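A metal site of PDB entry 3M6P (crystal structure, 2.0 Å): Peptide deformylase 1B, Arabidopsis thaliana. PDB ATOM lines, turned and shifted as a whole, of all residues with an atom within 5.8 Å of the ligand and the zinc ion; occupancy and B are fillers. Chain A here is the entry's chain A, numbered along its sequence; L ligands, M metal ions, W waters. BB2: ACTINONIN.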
ATOM      1  N   THR A  39      -2.695 -11.758  24.896  1.00  0.00           N
ATOM      2  CA  THR A  39      -2.279 -12.842  25.804  1.00  0.00           C
ATOM      3  C   THR A  39      -1.732 -14.046  25.051  1.00  0.00           C
ATOM      4  O   THR A  39      -1.499 -15.094  25.636  1.00  0.00           O
ATOM      5  CB  THR A  39      -3.455 -13.307  26.696  1.00  0.00           C
ATOM      6  OG1 THR A  39      -4.546 -13.750  25.843  1.00  0.00           O
ATOM      7  CG2 THR A  39      -3.891 -12.149  27.589  1.00  0.00           C
ATOM      8  N   ASP A  40      -1.546 -13.896  23.730  1.00  0.00           N
ATOM      9  CA  ASP A  40      -1.163 -15.012  22.844  1.00  0.00           C
ATOM     10  C   ASP A  40      -2.074 -16.258  22.868  1.00  0.00           C
ATOM     11  O   ASP A  40      -1.590 -17.405  22.742  1.00  0.00           O
ATOM     12  CB  ASP A  40       0.301 -15.421  23.127  1.00  0.00           C
ATOM     13  CG  ASP A  40       1.208 -14.254  23.123  1.00  0.00           C
ATOM     14  OD1 ASP A  40       1.099 -13.439  22.175  1.00  0.00           O
ATOM     15  OD2 ASP A  40       2.019 -14.121  24.080  1.00  0.00           O
ATOM     16  N   GLY A  41      -3.390 -16.031  22.915  1.00  0.00           N
ATOM     17  CA  GLY A  41      -4.368 -17.101  22.848  1.00  0.00           C
ATOM     18  C   GLY A  41      -4.771 -17.421  21.437  1.00  0.00           C
ATOM     19  O   GLY A  41      -4.398 -16.710  20.530  1.00  0.00           O
ATOM     20  N   ILE A  42      -5.524 -18.509  21.244  1.00  0.00           N
ATOM     21  CA  ILE A  42      -6.035 -18.864  19.946  1.00  0.00           C
ATOM     22  C   ILE A  42      -7.565 -18.923  19.988  1.00  0.00           C
ATOM     23  O   ILE A  42      -8.191 -19.269  19.026  1.00  0.00           O
ATOM     24  CB  ILE A  42      -5.416 -20.153  19.422  1.00  0.00           C
ATOM     25  CG1 ILE A  42      -5.796 -21.326  20.366  1.00  0.00           C
ATOM     26  CG2 ILE A  42      -3.844 -19.921  19.208  1.00  0.00           C
ATOM     27  CD1 ILE A  42      -5.090 -22.665  20.128  1.00  0.00           C
ATOM     28  N   GLY A  43      -8.132 -18.601  21.141  1.00  0.00           N
ATOM     29  CA  GLY A  43      -9.554 -18.380  21.323  1.00  0.00           C
ATOM     30  C   GLY A  43      -9.859 -17.750  22.665  1.00  0.00           C
ATOM     31  O   GLY A  43      -8.961 -17.623  23.534  1.00  0.00           O
ATOM     32  N   LEU A  44     -11.118 -17.329  22.810  1.00  0.00           N
ATOM     33  CA  LEU A  44     -11.643 -16.787  24.055  1.00  0.00           C
ATOM     34  C   LEU A  44     -13.118 -16.982  24.134  1.00  0.00           C
ATOM     35  O   LEU A  44     -13.842 -16.912  23.134  1.00  0.00           O
ATOM     36  CB  LEU A  44     -11.304 -15.255  24.241  1.00  0.00           C
ATOM     37  CG  LEU A  44     -11.315 -14.640  25.665  1.00  0.00           C
ATOM     38  CD1 LEU A  44     -10.332 -15.293  26.703  1.00  0.00           C
ATOM     39  CD2 LEU A  44     -10.983 -13.122  25.600  1.00  0.00           C
ATOM     40  N   SER A  45     -13.618 -17.178  25.358  1.00  0.00           N
ATOM     41  CA  SER A  45     -15.067 -17.194  25.547  1.00  0.00           C
ATOM     42  C   SER A  45     -15.480 -16.090  26.509  1.00  0.00           C
ATOM     43  O   SER A  45     -14.709 -15.702  27.399  1.00  0.00           O
ATOM     44  CB  SER A  45     -15.466 -18.540  26.082  1.00  0.00           C
ATOM     45  OG  SER A  45     -14.982 -18.673  27.409  1.00  0.00           O
ATOM     46  N   GLN A  48     -14.839 -15.767  30.327  1.00  0.00           N
ATOM     47  CA  GLN A  48     -13.432 -15.454  30.629  1.00  0.00           C
ATOM     48  C   GLN A  48     -13.104 -13.968  30.745  1.00  0.00           C
ATOM     49  O   GLN A  48     -12.036 -13.633  31.226  1.00  0.00           O
ATOM     50  CB  GLN A  48     -12.507 -16.102  29.631  1.00  0.00           C
ATOM     51  CG  GLN A  48     -12.590 -17.633  29.692  1.00  0.00           C
ATOM     52  CD  GLN A  48     -11.638 -18.296  28.712  1.00  0.00           C
ATOM     53  OE1 GLN A  48     -11.907 -18.363  27.520  1.00  0.00           O
ATOM     54  NE2 GLN A  48     -10.514 -18.787  29.227  1.00  0.00           N
ATOM     55  N   PHE A  87      -4.248 -33.763  22.734  1.00  0.00           N
ATOM     56  CA  PHE A  87      -3.623 -32.473  22.374  1.00  0.00           C
ATOM     57  C   PHE A  87      -3.348 -31.801  23.697  1.00  0.00           C
ATOM     58  O   PHE A  87      -4.162 -31.902  24.623  1.00  0.00           O
ATOM     59  CB  PHE A  87      -4.523 -31.609  21.494  1.00  0.00           C
ATOM     60  CG  PHE A  87      -3.818 -30.391  20.821  1.00  0.00           C
ATOM     61  CD1 PHE A  87      -2.868 -30.570  19.813  1.00  0.00           C
ATOM     62  CD2 PHE A  87      -4.139 -29.085  21.195  1.00  0.00           C
ATOM     63  CE1 PHE A  87      -2.254 -29.474  19.186  1.00  0.00           C
ATOM     64  CE2 PHE A  87      -3.516 -27.970  20.578  1.00  0.00           C
ATOM     65  CZ  PHE A  87      -2.591 -28.159  19.587  1.00  0.00           C
ATOM     66  N   ASP A  88      -2.183 -31.175  23.814  1.00  0.00           N
ATOM     67  CA  ASP A  88      -1.823 -30.414  25.004  1.00  0.00           C
ATOM     68  C   ASP A  88      -2.491 -29.054  24.982  1.00  0.00           C
ATOM     69  O   ASP A  88      -2.191 -28.219  24.135  1.00  0.00           O
ATOM     70  CB  ASP A  88      -0.318 -30.265  25.117  1.00  0.00           C
ATOM     71  CG  ASP A  88       0.341 -31.561  25.400  1.00  0.00           C
ATOM     72  OD1 ASP A  88       1.526 -31.564  25.798  1.00  0.00           O
ATOM     73  OD2 ASP A  88      -0.332 -32.608  25.239  1.00  0.00           O
ATOM     74  N   GLU A  89      -3.399 -28.862  25.936  1.00  0.00           N
ATOM     75  CA  GLU A  89      -4.132 -27.605  26.085  1.00  0.00           C
ATOM     76  C   GLU A  89      -3.614 -26.841  27.256  1.00  0.00           C
ATOM     77  O   GLU A  89      -3.211 -27.432  28.258  1.00  0.00           O
ATOM     78  CB  GLU A  89      -5.605 -27.883  26.366  1.00  0.00           C
ATOM     79  CG  GLU A  89      -6.186 -28.990  25.548  1.00  0.00           C
ATOM     80  CD  GLU A  89      -7.675 -28.853  25.316  1.00  0.00           C
ATOM     81  OE1 GLU A  89      -8.180 -29.599  24.453  1.00  0.00           O
ATOM     82  OE2 GLU A  89      -8.341 -28.023  26.002  1.00  0.00           O
ATOM     83  N   GLY A  90      -3.659 -25.517  27.117  1.00  0.00           N
ATOM     84  CA  GLY A  90      -3.563 -24.587  28.216  1.00  0.00           C
ATOM     85  C   GLY A  90      -4.834 -23.762  28.207  1.00  0.00           C
ATOM     86  O   GLY A  90      -5.593 -23.741  27.233  1.00  0.00           O
ATOM     87  N   CYS A  91      -5.000 -22.933  29.199  1.00  0.00           N
ATOM     88  CA  CYS A  91      -6.192 -22.127  29.221  1.00  0.00           C
ATOM     89  C   CYS A  91      -5.822 -20.829  29.854  1.00  0.00           C
ATOM     90  O   CYS A  91      -5.109 -20.801  30.854  1.00  0.00           O
ATOM     91  CB  CYS A  91      -7.300 -22.864  30.031  1.00  0.00           C
ATOM     92  SG  CYS A  91      -8.919 -22.042  30.162  1.00  0.00           S
ATOM     93  N   LEU A  92      -6.306 -19.736  29.266  1.00  0.00           N
ATOM     94  CA  LEU A  92      -6.061 -18.370  29.791  1.00  0.00           C
ATOM     95  C   LEU A  92      -6.596 -18.168  31.212  1.00  0.00           C
ATOM     96  O   LEU A  92      -6.133 -17.272  31.960  1.00  0.00           O
ATOM     97  CB  LEU A  92      -6.662 -17.328  28.847  1.00  0.00           C
ATOM     98  CG  LEU A  92      -5.766 -17.076  27.606  1.00  0.00           C
ATOM     99  CD1 LEU A  92      -6.401 -16.031  26.764  1.00  0.00           C
ATOM    100  CD2 LEU A  92      -4.366 -16.675  27.960  1.00  0.00           C
ATOM    101  N   SER A  93      -7.563 -18.990  31.602  1.00  0.00           N
ATOM    102  CA  SER A  93      -8.089 -18.913  32.965  1.00  0.00           C
ATOM    103  C   SER A  93      -7.285 -19.701  33.952  1.00  0.00           C
ATOM    104  O   SER A  93      -7.650 -19.789  35.110  1.00  0.00           O
ATOM    105  CB  SER A  93      -9.521 -19.388  33.044  1.00  0.00           C
ATOM    106  OG  SER A  93     -10.373 -18.415  32.429  1.00  0.00           O
ATOM    107  N   ILE A  97      -0.654 -23.340  33.162  1.00  0.00           N
ATOM    108  CA  ILE A  97      -0.993 -24.769  33.330  1.00  0.00           C
ATOM    109  C   ILE A  97      -1.274 -25.390  31.988  1.00  0.00           C
ATOM    110  O   ILE A  97      -2.132 -24.873  31.284  1.00  0.00           O
ATOM    111  CB  ILE A  97      -2.192 -24.979  34.321  1.00  0.00           C
ATOM    112  CG1 ILE A  97      -1.866 -24.368  35.709  1.00  0.00           C
ATOM    113  CG2 ILE A  97      -2.603 -26.527  34.396  1.00  0.00           C
ATOM    114  CD1 ILE A  97      -3.006 -24.481  36.676  1.00  0.00           C
ATOM    115  N   TYR A  98      -0.547 -26.444  31.608  1.00  0.00           N
ATOM    116  CA  TYR A  98      -0.678 -27.134  30.315  1.00  0.00           C
ATOM    117  C   TYR A  98      -0.799 -28.634  30.559  1.00  0.00           C
ATOM    118  O   TYR A  98      -0.077 -29.178  31.381  1.00  0.00           O
ATOM    119  CB  TYR A  98       0.543 -26.873  29.390  1.00  0.00           C
ATOM    120  CG  TYR A  98       0.748 -25.403  29.063  1.00  0.00           C
ATOM    121  CD1 TYR A  98       1.483 -24.566  29.906  1.00  0.00           C
ATOM    122  CD2 TYR A  98       0.173 -24.848  27.921  1.00  0.00           C
ATOM    123  CE1 TYR A  98       1.618 -23.191  29.647  1.00  0.00           C
ATOM    124  CE2 TYR A  98       0.318 -23.485  27.629  1.00  0.00           C
ATOM    125  CZ  TYR A  98       1.029 -22.655  28.503  1.00  0.00           C
ATOM    126  OH  TYR A  98       1.157 -21.294  28.197  1.00  0.00           O
ATOM    127  N   LEU A 126      -7.399 -28.138  14.332  1.00  0.00           N
ATOM    128  CA  LEU A 126      -7.292 -27.159  15.412  1.00  0.00           C
ATOM    129  C   LEU A 126      -8.629 -26.447  15.585  1.00  0.00           C
ATOM    130  O   LEU A 126      -9.122 -26.291  16.695  1.00  0.00           O
ATOM    131  CB  LEU A 126      -6.123 -26.189  15.171  1.00  0.00           C
ATOM    132  CG  LEU A 126      -5.542 -25.386  16.360  1.00  0.00           C
ATOM    133  CD1 LEU A 126      -5.118 -26.244  17.527  1.00  0.00           C
ATOM    134  CD2 LEU A 126      -4.368 -24.578  15.910  1.00  0.00           C
ATOM    135  N   ARG A 129     -10.695 -28.489  17.851  1.00  0.00           N
ATOM    136  CA  ARG A 129     -10.079 -28.535  19.183  1.00  0.00           C
ATOM    137  C   ARG A 129     -10.344 -27.204  20.000  1.00  0.00           C
ATOM    138  O   ARG A 129     -10.742 -27.229  21.159  1.00  0.00           O
ATOM    139  CB  ARG A 129      -8.599 -28.756  19.006  1.00  0.00           C
ATOM    140  CG  ARG A 129      -7.916 -29.029  20.303  1.00  0.00           C
ATOM    141  CD  ARG A 129      -8.707 -30.195  20.908  1.00  0.00           C
ATOM    142  NE  ARG A 129      -8.057 -30.760  22.028  1.00  0.00           N
ATOM    143  CZ  ARG A 129      -7.789 -32.016  22.226  1.00  0.00           C
ATOM    144  NH1 ARG A 129      -8.143 -32.967  21.371  1.00  0.00           N
ATOM    145  NH2 ARG A 129      -7.147 -32.292  23.350  1.00  0.00           N
ATOM    146  N   ILE A 130     -10.131 -26.067  19.367  1.00  0.00           N
ATOM    147  CA  ILE A 130     -10.350 -24.785  20.006  1.00  0.00           C
ATOM    148  C   ILE A 130     -11.839 -24.642  20.325  1.00  0.00           C
ATOM    149  O   ILE A 130     -12.222 -24.234  21.445  1.00  0.00           O
ATOM    150  CB  ILE A 130      -9.937 -23.625  19.071  1.00  0.00           C
ATOM    151  CG1 ILE A 130      -8.437 -23.670  18.743  1.00  0.00           C
ATOM    152  CG2 ILE A 130     -10.319 -22.301  19.682  1.00  0.00           C
ATOM    153  CD1 ILE A 130      -8.026 -22.680  17.630  1.00  0.00           C
ATOM    154  N   HIS A 133     -12.916 -26.823  23.346  1.00  0.00           N
ATOM    155  CA  HIS A 133     -12.411 -26.023  24.502  1.00  0.00           C
ATOM    156  C   HIS A 133     -13.307 -24.820  24.923  1.00  0.00           C
ATOM    157  O   HIS A 133     -13.694 -24.695  26.097  1.00  0.00           O
ATOM    158  CB  HIS A 133     -11.009 -25.509  24.254  1.00  0.00           C
ATOM    159  CG  HIS A 133     -10.381 -24.896  25.465  1.00  0.00           C
ATOM    160  ND1 HIS A 133      -9.429 -25.558  26.222  1.00  0.00           N
ATOM    161  CD2 HIS A 133     -10.555 -23.683  26.046  1.00  0.00           C
ATOM    162  CE1 HIS A 133      -9.040 -24.755  27.213  1.00  0.00           C
ATOM    163  NE2 HIS A 133      -9.742 -23.636  27.140  1.00  0.00           N
ATOM    164  N   GLU A 134     -13.650 -23.966  23.958  1.00  0.00           N
ATOM    165  CA  GLU A 134     -14.420 -22.729  24.215  1.00  0.00           C
ATOM    166  C   GLU A 134     -15.931 -23.029  24.437  1.00  0.00           C
ATOM    167  O   GLU A 134     -16.610 -22.364  25.206  1.00  0.00           O
ATOM    168  CB  GLU A 134     -14.320 -21.762  23.052  1.00  0.00           C
ATOM    169  CG  GLU A 134     -12.992 -21.335  22.550  1.00  0.00           C
ATOM    170  CD  GLU A 134     -12.123 -20.699  23.618  1.00  0.00           C
ATOM    171  OE1 GLU A 134     -12.656 -20.082  24.591  1.00  0.00           O
ATOM    172  OE2 GLU A 134     -10.888 -20.777  23.450  1.00  0.00           O
ATOM    173  N   HIS A 137     -16.465 -23.927  27.800  1.00  0.00           N
ATOM    174  CA  HIS A 137     -16.578 -22.742  28.626  1.00  0.00           C
ATOM    175  C   HIS A 137     -18.015 -22.194  28.636  1.00  0.00           C
ATOM    176  O   HIS A 137     -18.511 -21.708  29.661  1.00  0.00           O
ATOM    177  CB  HIS A 137     -15.624 -21.671  28.127  1.00  0.00           C
ATOM    178  CG  HIS A 137     -14.233 -21.752  28.704  1.00  0.00           C
ATOM    179  ND1 HIS A 137     -13.970 -21.541  30.035  1.00  0.00           N
ATOM    180  CD2 HIS A 137     -13.028 -21.840  28.089  1.00  0.00           C
ATOM    181  CE1 HIS A 137     -12.666 -21.622  30.252  1.00  0.00           C
ATOM    182  NE2 HIS A 137     -12.057 -21.737  29.085  1.00  0.00           N
HETATM  183  C5  BB2 L   1      -7.529 -19.713  25.381  1.00  0.00           C
HETATM  184  C3  BB2 L   1      -8.703 -20.122  26.209  1.00  0.00           C
HETATM  185  O4  BB2 L   1      -8.504 -20.456  27.352  1.00  0.00           O
HETATM  186  N1  BB2 L   1      -9.902 -20.134  25.619  1.00  0.00           N
HETATM  187  O2  BB2 L   1     -10.948 -20.538  26.406  1.00  0.00           O
HETATM  188  C6  BB2 L   1      -6.848 -21.069  25.133  1.00  0.00           C
HETATM  189  C12 BB2 L   1      -5.499 -20.864  24.524  1.00  0.00           C
HETATM  190  O13 BB2 L   1      -5.334 -20.035  23.624  1.00  0.00           O
HETATM  191  C7  BB2 L   1      -7.680 -21.887  24.042  1.00  0.00           C
HETATM  192  C8  BB2 L   1      -6.973 -23.218  23.627  1.00  0.00           C
HETATM  193  C9  BB2 L   1      -7.778 -23.951  22.587  1.00  0.00           C
HETATM  194  C10 BB2 L   1      -7.332 -25.478  22.583  1.00  0.00           C
HETATM  195  C11 BB2 L   1      -5.792 -25.674  22.471  1.00  0.00           C
HETATM  196  N14 BB2 L   1      -4.577 -21.637  25.017  1.00  0.00           N
HETATM  197  C15 BB2 L   1      -3.237 -21.612  24.466  1.00  0.00           C
HETATM  198  C16 BB2 L   1      -2.201 -21.086  25.461  1.00  0.00           C
HETATM  199  C18 BB2 L   1      -2.491 -19.575  25.734  1.00  0.00           C
HETATM  200  C17 BB2 L   1      -2.337 -21.811  26.750  1.00  0.00           C
HETATM  201  C19 BB2 L   1      -2.933 -23.052  23.950  1.00  0.00           C
HETATM  202  O20 BB2 L   1      -3.408 -24.046  24.527  1.00  0.00           O
HETATM  203  N21 BB2 L   1      -2.161 -23.216  22.834  1.00  0.00           N
HETATM  204  C22 BB2 L   1      -1.817 -24.518  22.262  1.00  0.00           C
HETATM  205  C23 BB2 L   1      -1.564 -22.120  22.040  1.00  0.00           C
HETATM  206  C24 BB2 L   1      -1.367 -22.739  20.655  1.00  0.00           C
HETATM  207  C25 BB2 L   1      -1.148 -24.217  20.921  1.00  0.00           C
HETATM  208  C26 BB2 L   1      -0.788 -25.272  23.148  1.00  0.00           C
HETATM  209  O27 BB2 L   1      -0.769 -26.622  22.662  1.00  0.00           O
HETATM  210 ZN    ZN M   1      -9.986 -21.667  28.248  1.00  0.00          ZN
HETATM  211  O   HOH W   1       0.867 -27.658  20.479  1.00  0.00           O
HETATM  212  O   HOH W   2       1.397 -20.837  19.981  1.00  0.00           O
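The backbone NH (N) of Leu 92 sits close to an oxygen (O4) of the ligand, at 3.0 Å.
The backbone NH (N) of Ile 42 lies within hydrogen-bond range of an oxygen (O13) of the ligand (2.8 Å).
O of Gly 43 lies close to N1 of the ligand (3.4 Å).
An oxygen (O20) of the ligand sits at hydrogen-bond distance from the backbone NH (N) of Gly 90, at 3.0 Å.
The backbone carbonyl oxygen (O) of Gly 90 lies within hydrogen-bond range of a nitrogen (N14) of the ligand.
OE1 of Gln 48 lies within hydrogen-bond range of N1 of the ligand.
An oxygen (O27) of the ligand sits at hydrogen-bond distance from the backbone carbonyl oxygen (O) of Asp 88, at 2.6 Å.
OE2 of Glu 134 is in hydrogen-bond range of N1 of the ligand (2.5 Å).
The side-chain carboxylate (OE1) of Glu 89 is in salt-bridge range of the guanidinium group (NE) of Arg 129 (2.7 Å).
The side-chain hydroxyl of Ser 93 sits at hydrogen-bond distance from the side-chain amide nitrogen of Gln 48, at 3.2 Å.
The side-chain sulfur (SG) of Cys 91 sits close to the backbone NH (N) of Ser 93 (3.6 Å).
A ring nitrogen (NE2) of His 137 sits close to the side-chain amide nitrogen (NE2) of Gln 48.
The backbone carbonyl oxygen (O) of Phe 87 is in hydrogen-bond range of the guanidinium group (NH2) of Arg 129.
The side-chain sulfur of Cys 91 lies close to the side-chain amide nitrogen of Gln 48 (3.7 Å).
A ring nitrogen (ND1) of His 133 sits at hydrogen-bond distance from the side-chain carboxylate of Glu 89 (2.7 Å).
The side-chain amide oxygen (OE1) of Gln 48 sits at hydrogen-bond distance from the backbone NH (N) of Ser 45 (3.0 Å).
O of Asp 40 touches C18 of the ligand, at 3.8 Å.
Gly 41 touches the ligand (CA to O13, 3.2 Å).
CE2 of Phe 87 touches O27 of the ligand, at 3.7 Å.
Glu 89 touches the ligand.
CE2 of Tyr 98 touches C17 of the ligand, 3.3 Å away.
Ile 130 touches the ligand (CA to C9, 3.7 Å).
Hydrophobic or aromatic side chains that line the ligand: Ile 42, Phe 87, Leu 92, Tyr 98, Ile 130, His 133 and His 137.
Merely in contact with the zinc ion: Gln 48.
Of the 23 residues printed, 4 come within 4 Å of the zinc ion.
The zinc ion is bound by O4 of the ligand, SG of Cys 91, NE2 of His 137, NE2 of His 133 and O2 of the ligand.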
